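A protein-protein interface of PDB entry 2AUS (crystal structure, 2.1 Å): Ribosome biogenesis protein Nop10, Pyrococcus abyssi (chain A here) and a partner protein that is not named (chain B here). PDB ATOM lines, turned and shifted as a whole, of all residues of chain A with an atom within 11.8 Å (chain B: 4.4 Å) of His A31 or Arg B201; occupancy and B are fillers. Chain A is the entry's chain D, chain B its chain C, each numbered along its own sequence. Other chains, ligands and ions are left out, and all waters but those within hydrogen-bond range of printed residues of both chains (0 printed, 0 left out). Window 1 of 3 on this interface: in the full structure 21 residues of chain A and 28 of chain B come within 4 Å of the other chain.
CG2 of Val B111 touches CD2 of Tyr A14, 3.8 Å away.
Thr B203 touches Tyr A14.
Ala A30 touches Ser B86.
Pro B55 touches His A31 (CD to ND1, 3.5 Å).
OG of Ser B86 touches CB of His A31, at 3.5 Å.
His A31 touches Arg B201 (CA to NH1, 3.9 Å).
Pro A32 touches Asp B52.
CD of Pro B55 touches O of Pro A32, 3.8 Å away.
Pro A32 touches Arg B201 (CD to NH1, 3.8 Å).
The backbone NH (N) of Ser B86 is in hydrogen-bond range of the backbone carbonyl oxygen (O) of Leu B200 (3.4 Å).
The side-chain carboxylate of Asp B52 lies within salt-bridge range of the guanidinium group of Arg B201, 2.8 Å away.
The backbone NH (N) of Lys A7 sits at hydrogen-bond distance from the backbone carbonyl oxygen (O) of Lys A28 (2.7 Å).
N of Gly B87 sits at hydrogen-bond distance from OD1 of Asp B52 (3.2 Å).
OG of Ser B86 lies within hydrogen-bond range of NH1 of Arg B201, at 3.2 Å.
The backbone NH of Val B111 sits at hydrogen-bond distance from the backbone carbonyl oxygen of Arg B201 (2.8 Å).
Of the 22 printed residues of chain A, 6 touch a printed residue of chain B.
Hydrophobic or aromatic side chains of chain A within 4 Å of the printed part of chain B: Tyr A14, His A31 and Pro A32.
Of the 13 printed residues of chain B, 7 touch a printed residue of chain A.
Hydrophobic or aromatic side chains of chain B within 4 Å of the printed part of chain A: Pro B55 and Val B111.
Among the printed residues, 14 pairs touch across the chains.
Among the printed residues, Asp or Glu carboxylates within 4 Å of a Lys or Arg side-chain nitrogen of the other chain: Lys A7 with Glu B210 (2.7 Å).
Cys A8 touches none of the printed residues of chain B.
Printed residues of chain B within 4 Å of Tyr A14: Val B111 (3.8 Å), Arg B201 (2.7 Å), Thr B203 (3.8 Å) and Glu B210 (2.5 Å).
Glu A18 touches none of the printed residues of chain B.
Of the printed residues of chain B, Ala A30 touches Ser B86 and Arg B201.
Printed residues of chain B within 4 Å of Pro A32: Asp B52 (3.2 Å), Pro B55 (3.8 Å) and Arg B201 (3.8 Å).
Of the printed residues of chain B, Arg A34 touches Pro B55.
Of chain A, only Pro A32 (3.2 Å) comes within 4 Å of Asp B52.
Of the printed residues of chain A, Pro B55 touches His A31, Pro A32 and Arg A34.
No residue of chain A comes within 4 Å of Val B85.
Of chain A, only Ala A30 and His A31 come within 4 Å of Ser B86.
No residue of chain A comes within 4 Å of Gly B87.
No residue of chain A comes within 4 Å of Tyr B110.
Val B111 touches one residue of chain A.
No residue of chain A comes within 4 Å of Leu B200.
Of chain A, only Tyr A14 (2.7 Å), Ala A30 (3.0 Å), His A31 (3.9 Å) and Pro A32 (3.8 Å) come within 4 Å of Arg B201.
Of chain A, only Tyr A14 (3.8 Å) comes within 4 Å of Thr B203.
The nearest printed residue of chain B that does not touch His A31 is Asp B52 (5.2 Å).
The guanidinium group (NH1) of Arg B201 lies close to the backbone carbonyl oxygen (O) of Ala A30 (3.4 Å).
The side-chain hydroxyl (OH) of Tyr A14 lies within hydrogen-bond range of the guanidinium group (NE) of Arg B201, at 2.7 Å.
The side-chain carboxylate (OE2) of Glu B210 is in salt-bridge range of the side-chain amino group (NZ) of Lys A7, at 2.7 Å.
The side-chain hydroxyl of Tyr A14 is in hydrogen-bond range of the side-chain carboxylate of Glu B210 (2.5 Å).
The backbone carbonyl oxygen (O) of Pro B55 is in hydrogen-bond range of the guanidinium group (NH1) of Arg A34, 3.2 Å away.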
ATOM      1  N   ARG A   4       6.291   8.571  12.224  1.00  0.00           N
ATOM      2  CA  ARG A   4       6.788   7.609  11.190  1.00  0.00           C
ATOM      3  C   ARG A   4       8.310   7.471  11.209  1.00  0.00           C
ATOM      4  O   ARG A   4       8.837   6.370  11.034  1.00  0.00           O
ATOM      5  CB  ARG A   4       6.344   8.045   9.787  1.00  0.00           C
ATOM      6  CG  ARG A   4       4.838   8.059   9.543  1.00  0.00           C
ATOM      7  CD  ARG A   4       4.249   6.656   9.534  1.00  0.00           C
ATOM      8  NE  ARG A   4       4.890   5.781   8.553  1.00  0.00           N
ATOM      9  CZ  ARG A   4       4.857   5.970   7.236  1.00  0.00           C
ATOM     10  NH1 ARG A   4       4.209   7.011   6.725  1.00  0.00           N
ATOM     11  NH2 ARG A   4       5.470   5.114   6.427  1.00  0.00           N
ATOM     12  N   ILE A   5       9.026   8.578  11.403  1.00  0.00           N
ATOM     13  CA  ILE A   5      10.485   8.513  11.441  1.00  0.00           C
ATOM     14  C   ILE A   5      10.922   7.912  12.773  1.00  0.00           C
ATOM     15  O   ILE A   5      10.606   8.447  13.832  1.00  0.00           O
ATOM     16  CB  ILE A   5      11.139   9.910  11.291  1.00  0.00           C
ATOM     17  CG1 ILE A   5      10.810  10.504   9.919  1.00  0.00           C
ATOM     18  CG2 ILE A   5      12.650   9.792  11.445  1.00  0.00           C
ATOM     19  CD1 ILE A   5      11.523  11.822   9.637  1.00  0.00           C
ATOM     20  N   ARG A   6      11.642   6.799  12.719  1.00  0.00           N
ATOM     21  CA  ARG A   6      12.098   6.139  13.939  1.00  0.00           C
ATOM     22  C   ARG A   6      13.620   6.001  13.962  1.00  0.00           C
ATOM     23  O   ARG A   6      14.283   6.156  12.935  1.00  0.00           O
ATOM     24  CB  ARG A   6      11.451   4.750  14.059  1.00  0.00           C
ATOM     25  CG  ARG A   6       9.928   4.735  13.884  1.00  0.00           C
ATOM     26  CD  ARG A   6       9.339   3.347  14.140  1.00  0.00           C
ATOM     27  NE  ARG A   6       9.370   2.991  15.559  1.00  0.00           N
ATOM     28  CZ  ARG A   6       8.484   3.415  16.457  1.00  0.00           C
ATOM     29  NH1 ARG A   6       7.484   4.207  16.089  1.00  0.00           N
ATOM     30  NH2 ARG A   6       8.605   3.062  17.730  1.00  0.00           N
ATOM     31  N   LYS A   7      14.167   5.715  15.140  1.00  0.00           N
ATOM     32  CA  LYS A   7      15.608   5.541  15.295  1.00  0.00           C
ATOM     33  C   LYS A   7      15.916   4.429  16.290  1.00  0.00           C
ATOM     34  O   LYS A   7      15.172   4.217  17.247  1.00  0.00           O
ATOM     35  CB  LYS A   7      16.270   6.835  15.782  1.00  0.00           C
ATOM     36  CG  LYS A   7      17.787   6.730  15.873  1.00  0.00           C
ATOM     37  CD  LYS A   7      18.401   7.822  16.734  1.00  0.00           C
ATOM     38  CE  LYS A   7      18.281   9.188  16.093  1.00  0.00           C
ATOM     39  NZ  LYS A   7      18.897  10.246  16.941  1.00  0.00           N
ATOM     40  N   CYS A   8      17.018   3.722  16.054  1.00  0.00           N
ATOM     41  CA  CYS A   8      17.440   2.643  16.938  1.00  0.00           C
ATOM     42  C   CYS A   8      18.322   3.206  18.054  1.00  0.00           C
ATOM     43  O   CYS A   8      19.326   3.875  17.790  1.00  0.00           O
ATOM     44  CB  CYS A   8      18.221   1.580  16.156  1.00  0.00           C
ATOM     45  SG  CYS A   8      18.847   0.210  17.177  1.00  0.00           S
ATOM     46  N   PRO A   9      17.952   2.946  19.320  1.00  0.00           N
ATOM     47  CA  PRO A   9      18.704   3.424  20.485  1.00  0.00           C
ATOM     48  C   PRO A   9      20.179   3.024  20.447  1.00  0.00           C
ATOM     49  O   PRO A   9      21.018   3.654  21.089  1.00  0.00           O
ATOM     50  CB  PRO A   9      17.964   2.781  21.655  1.00  0.00           C
ATOM     51  CG  PRO A   9      16.551   2.715  21.159  1.00  0.00           C
ATOM     52  CD  PRO A   9      16.738   2.223  19.743  1.00  0.00           C
ATOM     53  N   CYS A  11      22.767   1.829  17.340  1.00  0.00           N
ATOM     54  CA  CYS A  11      23.575   2.499  16.324  1.00  0.00           C
ATOM     55  C   CYS A  11      23.028   3.865  15.913  1.00  0.00           C
ATOM     56  O   CYS A  11      23.666   4.591  15.145  1.00  0.00           O
ATOM     57  CB  CYS A  11      23.721   1.606  15.087  1.00  0.00           C
ATOM     58  SG  CYS A  11      22.160   1.092  14.329  1.00  0.00           S
ATOM     59  N   GLY A  12      21.851   4.214  16.428  1.00  0.00           N
ATOM     60  CA  GLY A  12      21.250   5.498  16.106  1.00  0.00           C
ATOM     61  C   GLY A  12      20.773   5.583  14.669  1.00  0.00           C
ATOM     62  O   GLY A  12      20.629   6.674  14.110  1.00  0.00           O
ATOM     63  N   ARG A  13      20.526   4.421  14.076  1.00  0.00           N
ATOM     64  CA  ARG A  13      20.062   4.322  12.697  1.00  0.00           C
ATOM     65  C   ARG A  13      18.638   4.847  12.542  1.00  0.00           C
ATOM     66  O   ARG A  13      17.769   4.558  13.363  1.00  0.00           O
ATOM     67  CB  ARG A  13      20.122   2.858  12.248  1.00  0.00           C
ATOM     68  CG  ARG A  13      19.304   2.518  11.009  1.00  0.00           C
ATOM     69  CD  ARG A  13      19.882   3.139   9.749  1.00  0.00           C
ATOM     70  NE  ARG A  13      19.179   2.679   8.554  1.00  0.00           N
ATOM     71  CZ  ARG A  13      19.494   3.042   7.314  1.00  0.00           C
ATOM     72  NH1 ARG A  13      20.503   3.878   7.099  1.00  0.00           N
ATOM     73  NH2 ARG A  13      18.798   2.571   6.287  1.00  0.00           N
ATOM     74  N   TYR A  14      18.413   5.636  11.498  1.00  0.00           N
ATOM     75  CA  TYR A  14      17.082   6.160  11.223  1.00  0.00           C
ATOM     76  C   TYR A  14      16.394   5.146  10.319  1.00  0.00           C
ATOM     77  O   TYR A  14      17.003   4.621   9.384  1.00  0.00           O
ATOM     78  CB  TYR A  14      17.157   7.526  10.533  1.00  0.00           C
ATOM     79  CG  TYR A  14      17.401   8.668  11.492  1.00  0.00           C
ATOM     80  CD1 TYR A  14      16.393   9.117  12.339  1.00  0.00           C
ATOM     81  CD2 TYR A  14      18.655   9.273  11.579  1.00  0.00           C
ATOM     82  CE1 TYR A  14      16.628  10.144  13.253  1.00  0.00           C
ATOM     83  CE2 TYR A  14      18.903  10.295  12.490  1.00  0.00           C
ATOM     84  CZ  TYR A  14      17.886  10.726  13.324  1.00  0.00           C
ATOM     85  OH  TYR A  14      18.117  11.737  14.229  1.00  0.00           O
ATOM     86  N   THR A  15      15.129   4.866  10.613  1.00  0.00           N
ATOM     87  CA  THR A  15      14.367   3.897   9.842  1.00  0.00           C
ATOM     88  C   THR A  15      12.881   4.132  10.049  1.00  0.00           C
ATOM     89  O   THR A  15      12.483   4.864  10.949  1.00  0.00           O
ATOM     90  CB  THR A  15      14.702   2.457  10.303  1.00  0.00           C
ATOM     91  OG1 THR A  15      13.873   1.516   9.609  1.00  0.00           O
ATOM     92  CG2 THR A  15      14.465   2.317  11.807  1.00  0.00           C
ATOM     93  N   LEU A  16      12.063   3.514   9.208  1.00  0.00           N
ATOM     94  CA  LEU A  16      10.621   3.644   9.336  1.00  0.00           C
ATOM     95  C   LEU A  16      10.103   2.374  10.003  1.00  0.00           C
ATOM     96  O   LEU A  16       8.986   2.339  10.518  1.00  0.00           O
ATOM     97  CB  LEU A  16       9.975   3.801   7.959  1.00  0.00           C
ATOM     98  CG  LEU A  16      10.393   5.003   7.113  1.00  0.00           C
ATOM     99  CD1 LEU A  16       9.716   4.914   5.750  1.00  0.00           C
ATOM    100  CD2 LEU A  16      10.012   6.293   7.820  1.00  0.00           C
ATOM    101  N   GLU A  18       9.742  -0.907  12.607  1.00  0.00           N
ATOM    102  CA  GLU A  18       9.563  -1.076  14.047  1.00  0.00           C
ATOM    103  C   GLU A  18      10.773  -1.745  14.683  1.00  0.00           C
ATOM    104  O   GLU A  18      11.053  -1.556  15.865  1.00  0.00           O
ATOM    105  CB  GLU A  18       8.318  -1.918  14.327  1.00  0.00           C
ATOM    106  CG  GLU A  18       7.030  -1.128  14.331  1.00  0.00           C
ATOM    107  CD  GLU A  18       7.111   0.069  15.252  1.00  0.00           C
ATOM    108  OE1 GLU A  18       7.613  -0.092  16.388  1.00  0.00           O
ATOM    109  OE2 GLU A  18       6.671   1.166  14.845  1.00  0.00           O
ATOM    110  N   THR A  27      12.764  -0.067  17.539  1.00  0.00           N
ATOM    111  CA  THR A  27      13.143   1.325  17.338  1.00  0.00           C
ATOM    112  C   THR A  27      12.130   2.246  18.010  1.00  0.00           C
ATOM    113  O   THR A  27      11.013   1.830  18.320  1.00  0.00           O
ATOM    114  CB  THR A  27      13.197   1.673  15.834  1.00  0.00           C
ATOM    115  OG1 THR A  27      11.893   1.509  15.261  1.00  0.00           O
ATOM    116  CG2 THR A  27      14.184   0.766  15.109  1.00  0.00           C
ATOM    117  N   LYS A  28      12.524   3.495  18.238  1.00  0.00           N
ATOM    118  CA  LYS A  28      11.629   4.462  18.862  1.00  0.00           C
ATOM    119  C   LYS A  28      11.505   5.722  18.008  1.00  0.00           C
ATOM    120  O   LYS A  28      12.375   6.008  17.184  1.00  0.00           O
ATOM    121  CB  LYS A  28      12.133   4.831  20.258  1.00  0.00           C
ATOM    122  CG  LYS A  28      11.159   5.700  21.038  1.00  0.00           C
ATOM    123  CD  LYS A  28       9.797   5.021  21.166  1.00  0.00           C
ATOM    124  CE  LYS A  28       8.748   5.984  21.698  1.00  0.00           C
ATOM    125  NZ  LYS A  28       9.184   6.612  22.972  1.00  0.00           N
ATOM    126  N   VAL A  29      10.421   6.470  18.205  1.00  0.00           N
ATOM    127  CA  VAL A  29      10.202   7.697  17.448  1.00  0.00           C
ATOM    128  C   VAL A  29      11.441   8.590  17.497  1.00  0.00           C
ATOM    129  O   VAL A  29      11.976   8.876  18.568  1.00  0.00           O
ATOM    130  CB  VAL A  29       8.978   8.480  17.982  1.00  0.00           C
ATOM    131  CG1 VAL A  29       7.731   7.624  17.851  1.00  0.00           C
ATOM    132  CG2 VAL A  29       9.198   8.887  19.434  1.00  0.00           C
ATOM    133  N   ALA A  30      11.891   9.015  16.320  1.00  0.00           N
ATOM    134  CA  ALA A  30      13.076   9.856  16.183  1.00  0.00           C
ATOM    135  C   ALA A  30      12.847  11.316  16.548  1.00  0.00           C
ATOM    136  O   ALA A  30      13.126  12.211  15.752  1.00  0.00           O
ATOM    137  CB  ALA A  30      13.611   9.764  14.761  1.00  0.00           C
ATOM    138  N   HIS A  31      12.325  11.558  17.744  1.00  0.00           N
ATOM    139  CA  HIS A  31      12.104  12.917  18.210  1.00  0.00           C
ATOM    140  C   HIS A  31      11.875  12.879  19.708  1.00  0.00           C
ATOM    141  O   HIS A  31      11.291  11.931  20.233  1.00  0.00           O
ATOM    142  CB  HIS A  31      10.924  13.579  17.476  1.00  0.00           C
ATOM    143  CG  HIS A  31       9.575  13.072  17.881  1.00  0.00           C
ATOM    144  ND1 HIS A  31       9.023  13.325  19.118  1.00  0.00           N
ATOM    145  CD2 HIS A  31       8.645  12.366  17.192  1.00  0.00           C
ATOM    146  CE1 HIS A  31       7.811  12.802  19.173  1.00  0.00           C
ATOM    147  NE2 HIS A  31       7.558  12.215  18.016  1.00  0.00           N
ATOM    148  N   PRO A  32      12.357  13.907  20.421  1.00  0.00           N
ATOM    149  CA  PRO A  32      12.215  13.997  21.874  1.00  0.00           C
ATOM    150  C   PRO A  32      10.773  14.142  22.340  1.00  0.00           C
ATOM    151  O   PRO A  32       9.918  14.655  21.617  1.00  0.00           O
ATOM    152  CB  PRO A  32      13.067  15.214  22.223  1.00  0.00           C
ATOM    153  CG  PRO A  32      12.851  16.098  21.038  1.00  0.00           C
ATOM    154  CD  PRO A  32      12.989  15.126  19.885  1.00  0.00           C
ATOM    155  N   PRO A  33      10.488  13.679  23.565  1.00  0.00           N
ATOM    156  CA  PRO A  33       9.150  13.750  24.152  1.00  0.00           C
ATOM    157  C   PRO A  33       8.604  15.171  24.164  1.00  0.00           C
ATOM    158  O   PRO A  33       9.364  16.140  24.205  1.00  0.00           O
ATOM    159  CB  PRO A  33       9.371  13.214  25.564  1.00  0.00           C
ATOM    160  CG  PRO A  33      10.464  12.218  25.372  1.00  0.00           C
ATOM    161  CD  PRO A  33      11.411  12.950  24.452  1.00  0.00           C
ATOM    162  N   ARG A  34       7.282  15.287  24.125  1.00  0.00           N
ATOM    163  CA  ARG A  34       6.629  16.588  24.161  1.00  0.00           C
ATOM    164  C   ARG A  34       6.983  17.206  25.513  1.00  0.00           C
ATOM    165  O   ARG A  34       7.148  16.489  26.500  1.00  0.00           O
ATOM    166  CB  ARG A  34       5.113  16.415  24.060  1.00  0.00           C
ATOM    167  CG  ARG A  34       4.650  15.484  22.938  1.00  0.00           C
ATOM    168  CD  ARG A  34       4.659  16.158  21.574  1.00  0.00           C
ATOM    169  NE  ARG A  34       4.172  15.258  20.532  1.00  0.00           N
ATOM    170  CZ  ARG A  34       3.902  15.625  19.281  1.00  0.00           C
ATOM    171  NH1 ARG A  34       4.064  16.887  18.900  1.00  0.00           N
ATOM    172  NH2 ARG A  34       3.473  14.723  18.404  1.00  0.00           N
ATOM    173  N   PHE A  35       7.107  18.525  25.567  1.00  0.00           N
ATOM    174  CA  PHE A  35       7.438  19.174  26.828  1.00  0.00           C
ATOM    175  C   PHE A  35       6.209  19.854  27.406  1.00  0.00           C
ATOM    176  O   PHE A  35       5.343  20.323  26.667  1.00  0.00           O
ATOM    177  CB  PHE A  35       8.546  20.210  26.627  1.00  0.00           C
ATOM    178  CG  PHE A  35       9.042  20.825  27.908  1.00  0.00           C
ATOM    179  CD1 PHE A  35       9.770  20.068  28.821  1.00  0.00           C
ATOM    180  CD2 PHE A  35       8.758  22.150  28.215  1.00  0.00           C
ATOM    181  CE1 PHE A  35      10.213  20.624  30.017  1.00  0.00           C
ATOM    182  CE2 PHE A  35       9.197  22.716  29.408  1.00  0.00           C
ATOM    183  CZ  PHE A  35       9.922  21.952  30.312  1.00  0.00           C
ATOM    184  N   ASP B  52      17.746  19.428  21.402  1.00  0.00           N
ATOM    185  CA  ASP B  52      16.980  18.594  20.475  1.00  0.00           C
ATOM    186  C   ASP B  52      15.574  19.144  20.621  1.00  0.00           C
ATOM    187  O   ASP B  52      14.867  18.811  21.574  1.00  0.00           O
ATOM    188  CB  ASP B  52      16.985  17.120  20.902  1.00  0.00           C
ATOM    189  CG  ASP B  52      16.349  16.195  19.855  1.00  0.00           C
ATOM    190  OD1 ASP B  52      15.585  16.680  18.991  1.00  0.00           O
ATOM    191  OD2 ASP B  52      16.612  14.973  19.896  1.00  0.00           O
ATOM    192  N   PRO B  55       8.977  18.269  18.571  1.00  0.00           N
ATOM    193  CA  PRO B  55       7.993  18.744  17.593  1.00  0.00           C
ATOM    194  C   PRO B  55       6.803  19.339  18.344  1.00  0.00           C
ATOM    195  O   PRO B  55       6.481  18.904  19.453  1.00  0.00           O
ATOM    196  CB  PRO B  55       7.617  17.475  16.841  1.00  0.00           C
ATOM    197  CG  PRO B  55       7.693  16.433  17.915  1.00  0.00           C
ATOM    198  CD  PRO B  55       8.988  16.795  18.632  1.00  0.00           C
ATOM    199  N   VAL B  85       8.862  20.545  13.098  1.00  0.00           N
ATOM    200  CA  VAL B  85      10.205  19.989  12.963  1.00  0.00           C
ATOM    201  C   VAL B  85      10.943  19.796  14.289  1.00  0.00           C
ATOM    202  O   VAL B  85      10.857  20.624  15.190  1.00  0.00           O
ATOM    203  CB  VAL B  85      11.067  20.881  12.044  1.00  0.00           C
ATOM    204  CG1 VAL B  85      12.436  20.226  11.801  1.00  0.00           C
ATOM    205  CG2 VAL B  85      10.335  21.118  10.728  1.00  0.00           C
ATOM    206  N   SER B  86      11.672  18.694  14.401  1.00  0.00           N
ATOM    207  CA  SER B  86      12.430  18.420  15.618  1.00  0.00           C
ATOM    208  C   SER B  86      13.923  18.393  15.292  1.00  0.00           C
ATOM    209  O   SER B  86      14.318  18.539  14.134  1.00  0.00           O
ATOM    210  CB  SER B  86      12.008  17.073  16.213  1.00  0.00           C
ATOM    211  OG  SER B  86      12.482  16.003  15.420  1.00  0.00           O
ATOM    212  N   GLY B  87      14.751  18.208  16.317  1.00  0.00           N
ATOM    213  CA  GLY B  87      16.182  18.134  16.088  1.00  0.00           C
ATOM    214  C   GLY B  87      17.047  19.283  16.583  1.00  0.00           C
ATOM    215  O   GLY B  87      16.611  20.166  17.325  1.00  0.00           O
ATOM    216  N   TYR B 110      19.545  17.248   7.403  1.00  0.00           N
ATOM    217  CA  TYR B 110      18.224  16.870   7.872  1.00  0.00           C
ATOM    218  C   TYR B 110      17.948  15.425   7.510  1.00  0.00           C
ATOM    219  O   TYR B 110      18.614  14.838   6.656  1.00  0.00           O
ATOM    220  CB  TYR B 110      17.157  17.718   7.184  1.00  0.00           C
ATOM    221  CG  TYR B 110      17.198  19.197   7.469  1.00  0.00           C
ATOM    222  CD1 TYR B 110      16.421  19.751   8.481  1.00  0.00           C
ATOM    223  CD2 TYR B 110      17.981  20.054   6.694  1.00  0.00           C
ATOM    224  CE1 TYR B 110      16.411  21.120   8.714  1.00  0.00           C
ATOM    225  CE2 TYR B 110      17.980  21.429   6.921  1.00  0.00           C
ATOM    226  CZ  TYR B 110      17.191  21.956   7.933  1.00  0.00           C
ATOM    227  OH  TYR B 110      17.176  23.315   8.171  1.00  0.00           O
ATOM    228  N   VAL B 111      16.962  14.854   8.183  1.00  0.00           N
ATOM    229  CA  VAL B 111      16.504  13.517   7.871  1.00  0.00           C
ATOM    230  C   VAL B 111      15.042  13.806   7.596  1.00  0.00           C
ATOM    231  O   VAL B 111      14.360  14.423   8.414  1.00  0.00           O
ATOM    232  CB  VAL B 111      16.662  12.544   9.045  1.00  0.00           C
ATOM    233  CG1 VAL B 111      15.896  11.253   8.752  1.00  0.00           C
ATOM    234  CG2 VAL B 111      18.131  12.215   9.223  1.00  0.00           C
ATOM    235  N   LEU B 200      10.079  16.037   9.274  1.00  0.00           N
ATOM    236  CA  LEU B 200      11.408  16.603   9.107  1.00  0.00           C
ATOM    237  C   LEU B 200      12.132  16.701  10.448  1.00  0.00           C
ATOM    238  O   LEU B 200      11.545  17.109  11.443  1.00  0.00           O
ATOM    239  CB  LEU B 200      11.292  18.004   8.504  1.00  0.00           C
ATOM    240  CG  LEU B 200      12.420  18.556   7.627  1.00  0.00           C
ATOM    241  CD1 LEU B 200      12.647  20.007   7.990  1.00  0.00           C
ATOM    242  CD2 LEU B 200      13.694  17.742   7.789  1.00  0.00           C
ATOM    243  N   ARG B 201      13.408  16.336  10.462  1.00  0.00           N
ATOM    244  CA  ARG B 201      14.216  16.409  11.673  1.00  0.00           C
ATOM    245  C   ARG B 201      15.604  16.920  11.303  1.00  0.00           C
ATOM    246  O   ARG B 201      16.266  16.359  10.429  1.00  0.00           O
ATOM    247  CB  ARG B 201      14.341  15.028  12.323  1.00  0.00           C
ATOM    248  CG  ARG B 201      15.236  15.009  13.566  1.00  0.00           C
ATOM    249  CD  ARG B 201      15.324  13.617  14.178  1.00  0.00           C
ATOM    250  NE  ARG B 201      16.344  13.538  15.225  1.00  0.00           N
ATOM    251  CZ  ARG B 201      16.241  14.113  16.422  1.00  0.00           C
ATOM    252  NH1 ARG B 201      15.159  14.811  16.730  1.00  0.00           N
ATOM    253  NH2 ARG B 201      17.225  13.995  17.312  1.00  0.00           N
ATOM    254  N   ARG B 202      16.040  17.995  11.951  1.00  0.00           N
ATOM    255  CA  ARG B 202      17.362  18.530  11.673  1.00  0.00           C
ATOM    256  C   ARG B 202      18.364  17.714  12.484  1.00  0.00           C
ATOM    257  O   ARG B 202      18.221  17.559  13.696  1.00  0.00           O
ATOM    258  CB  ARG B 202      17.450  20.002  12.067  1.00  0.00           C
ATOM    259  CG  ARG B 202      18.821  20.613  11.790  1.00  0.00           C
ATOM    260  CD  ARG B 202      18.996  21.928  12.527  1.00  0.00           C
ATOM    261  NE  ARG B 202      18.411  23.034  11.794  1.00  0.00           N
ATOM    262  CZ  ARG B 202      18.210  24.247  12.286  1.00  0.00           C
ATOM    263  NH1 ARG B 202      18.538  24.537  13.538  1.00  0.00           N
ATOM    264  NH2 ARG B 202      17.693  25.177  11.502  1.00  0.00           N
ATOM    265  N   THR B 203      19.373  17.188  11.805  1.00  0.00           N
ATOM    266  CA  THR B 203      20.376  16.370  12.461  1.00  0.00           C
ATOM    267  C   THR B 203      21.700  17.087  12.577  1.00  0.00           C
ATOM    268  O   THR B 203      22.629  16.574  13.191  1.00  0.00           O
ATOM    269  CB  THR B 203      20.600  15.056  11.700  1.00  0.00           C
ATOM    270  OG1 THR B 203      21.004  15.345  10.354  1.00  0.00           O
ATOM    271  CG2 THR B 203      19.320  14.229  11.689  1.00  0.00           C
ATOM    272  N   GLU B 210      24.030  15.519  16.319  1.00  0.00           N
ATOM    273  CA  GLU B 210      23.532  14.521  17.257  1.00  0.00           C
ATOM    274  C   GLU B 210      24.675  13.720  17.855  1.00  0.00           C
ATOM    275  O   GLU B 210      25.044  12.659  17.348  1.00  0.00           O
ATOM    276  CB  GLU B 210      22.558  13.573  16.559  1.00  0.00           C
ATOM    277  CG  GLU B 210      21.229  14.203  16.204  1.00  0.00           C
ATOM    278  CD  GLU B 210      20.250  13.185  15.665  1.00  0.00           C
ATOM    279  OE1 GLU B 210      20.420  12.739  14.511  1.00  0.00           O
ATOM    280  OE2 GLU B 210      19.314  12.820  16.399  1.00  0.00           O
ATOM    281  N   LEU B 214      23.987  16.726  22.538  1.00  0.00           N
ATOM    282  CA  LEU B 214      22.583  16.983  22.236  1.00  0.00           C
ATOM    283  C   LEU B 214      21.763  16.687  23.480  1.00  0.00           C
ATOM    284  O   LEU B 214      21.782  15.567  23.982  1.00  0.00           O
ATOM    285  CB  LEU B 214      22.099  16.093  21.089  1.00  0.00           C
ATOM    286  CG  LEU B 214      20.647  16.341  20.658  1.00  0.00           C
ATOM    287  CD1 LEU B 214      20.541  17.705  19.982  1.00  0.00           C
ATOM    288  CD2 LEU B 214      20.185  15.238  19.706  1.00  0.00           C
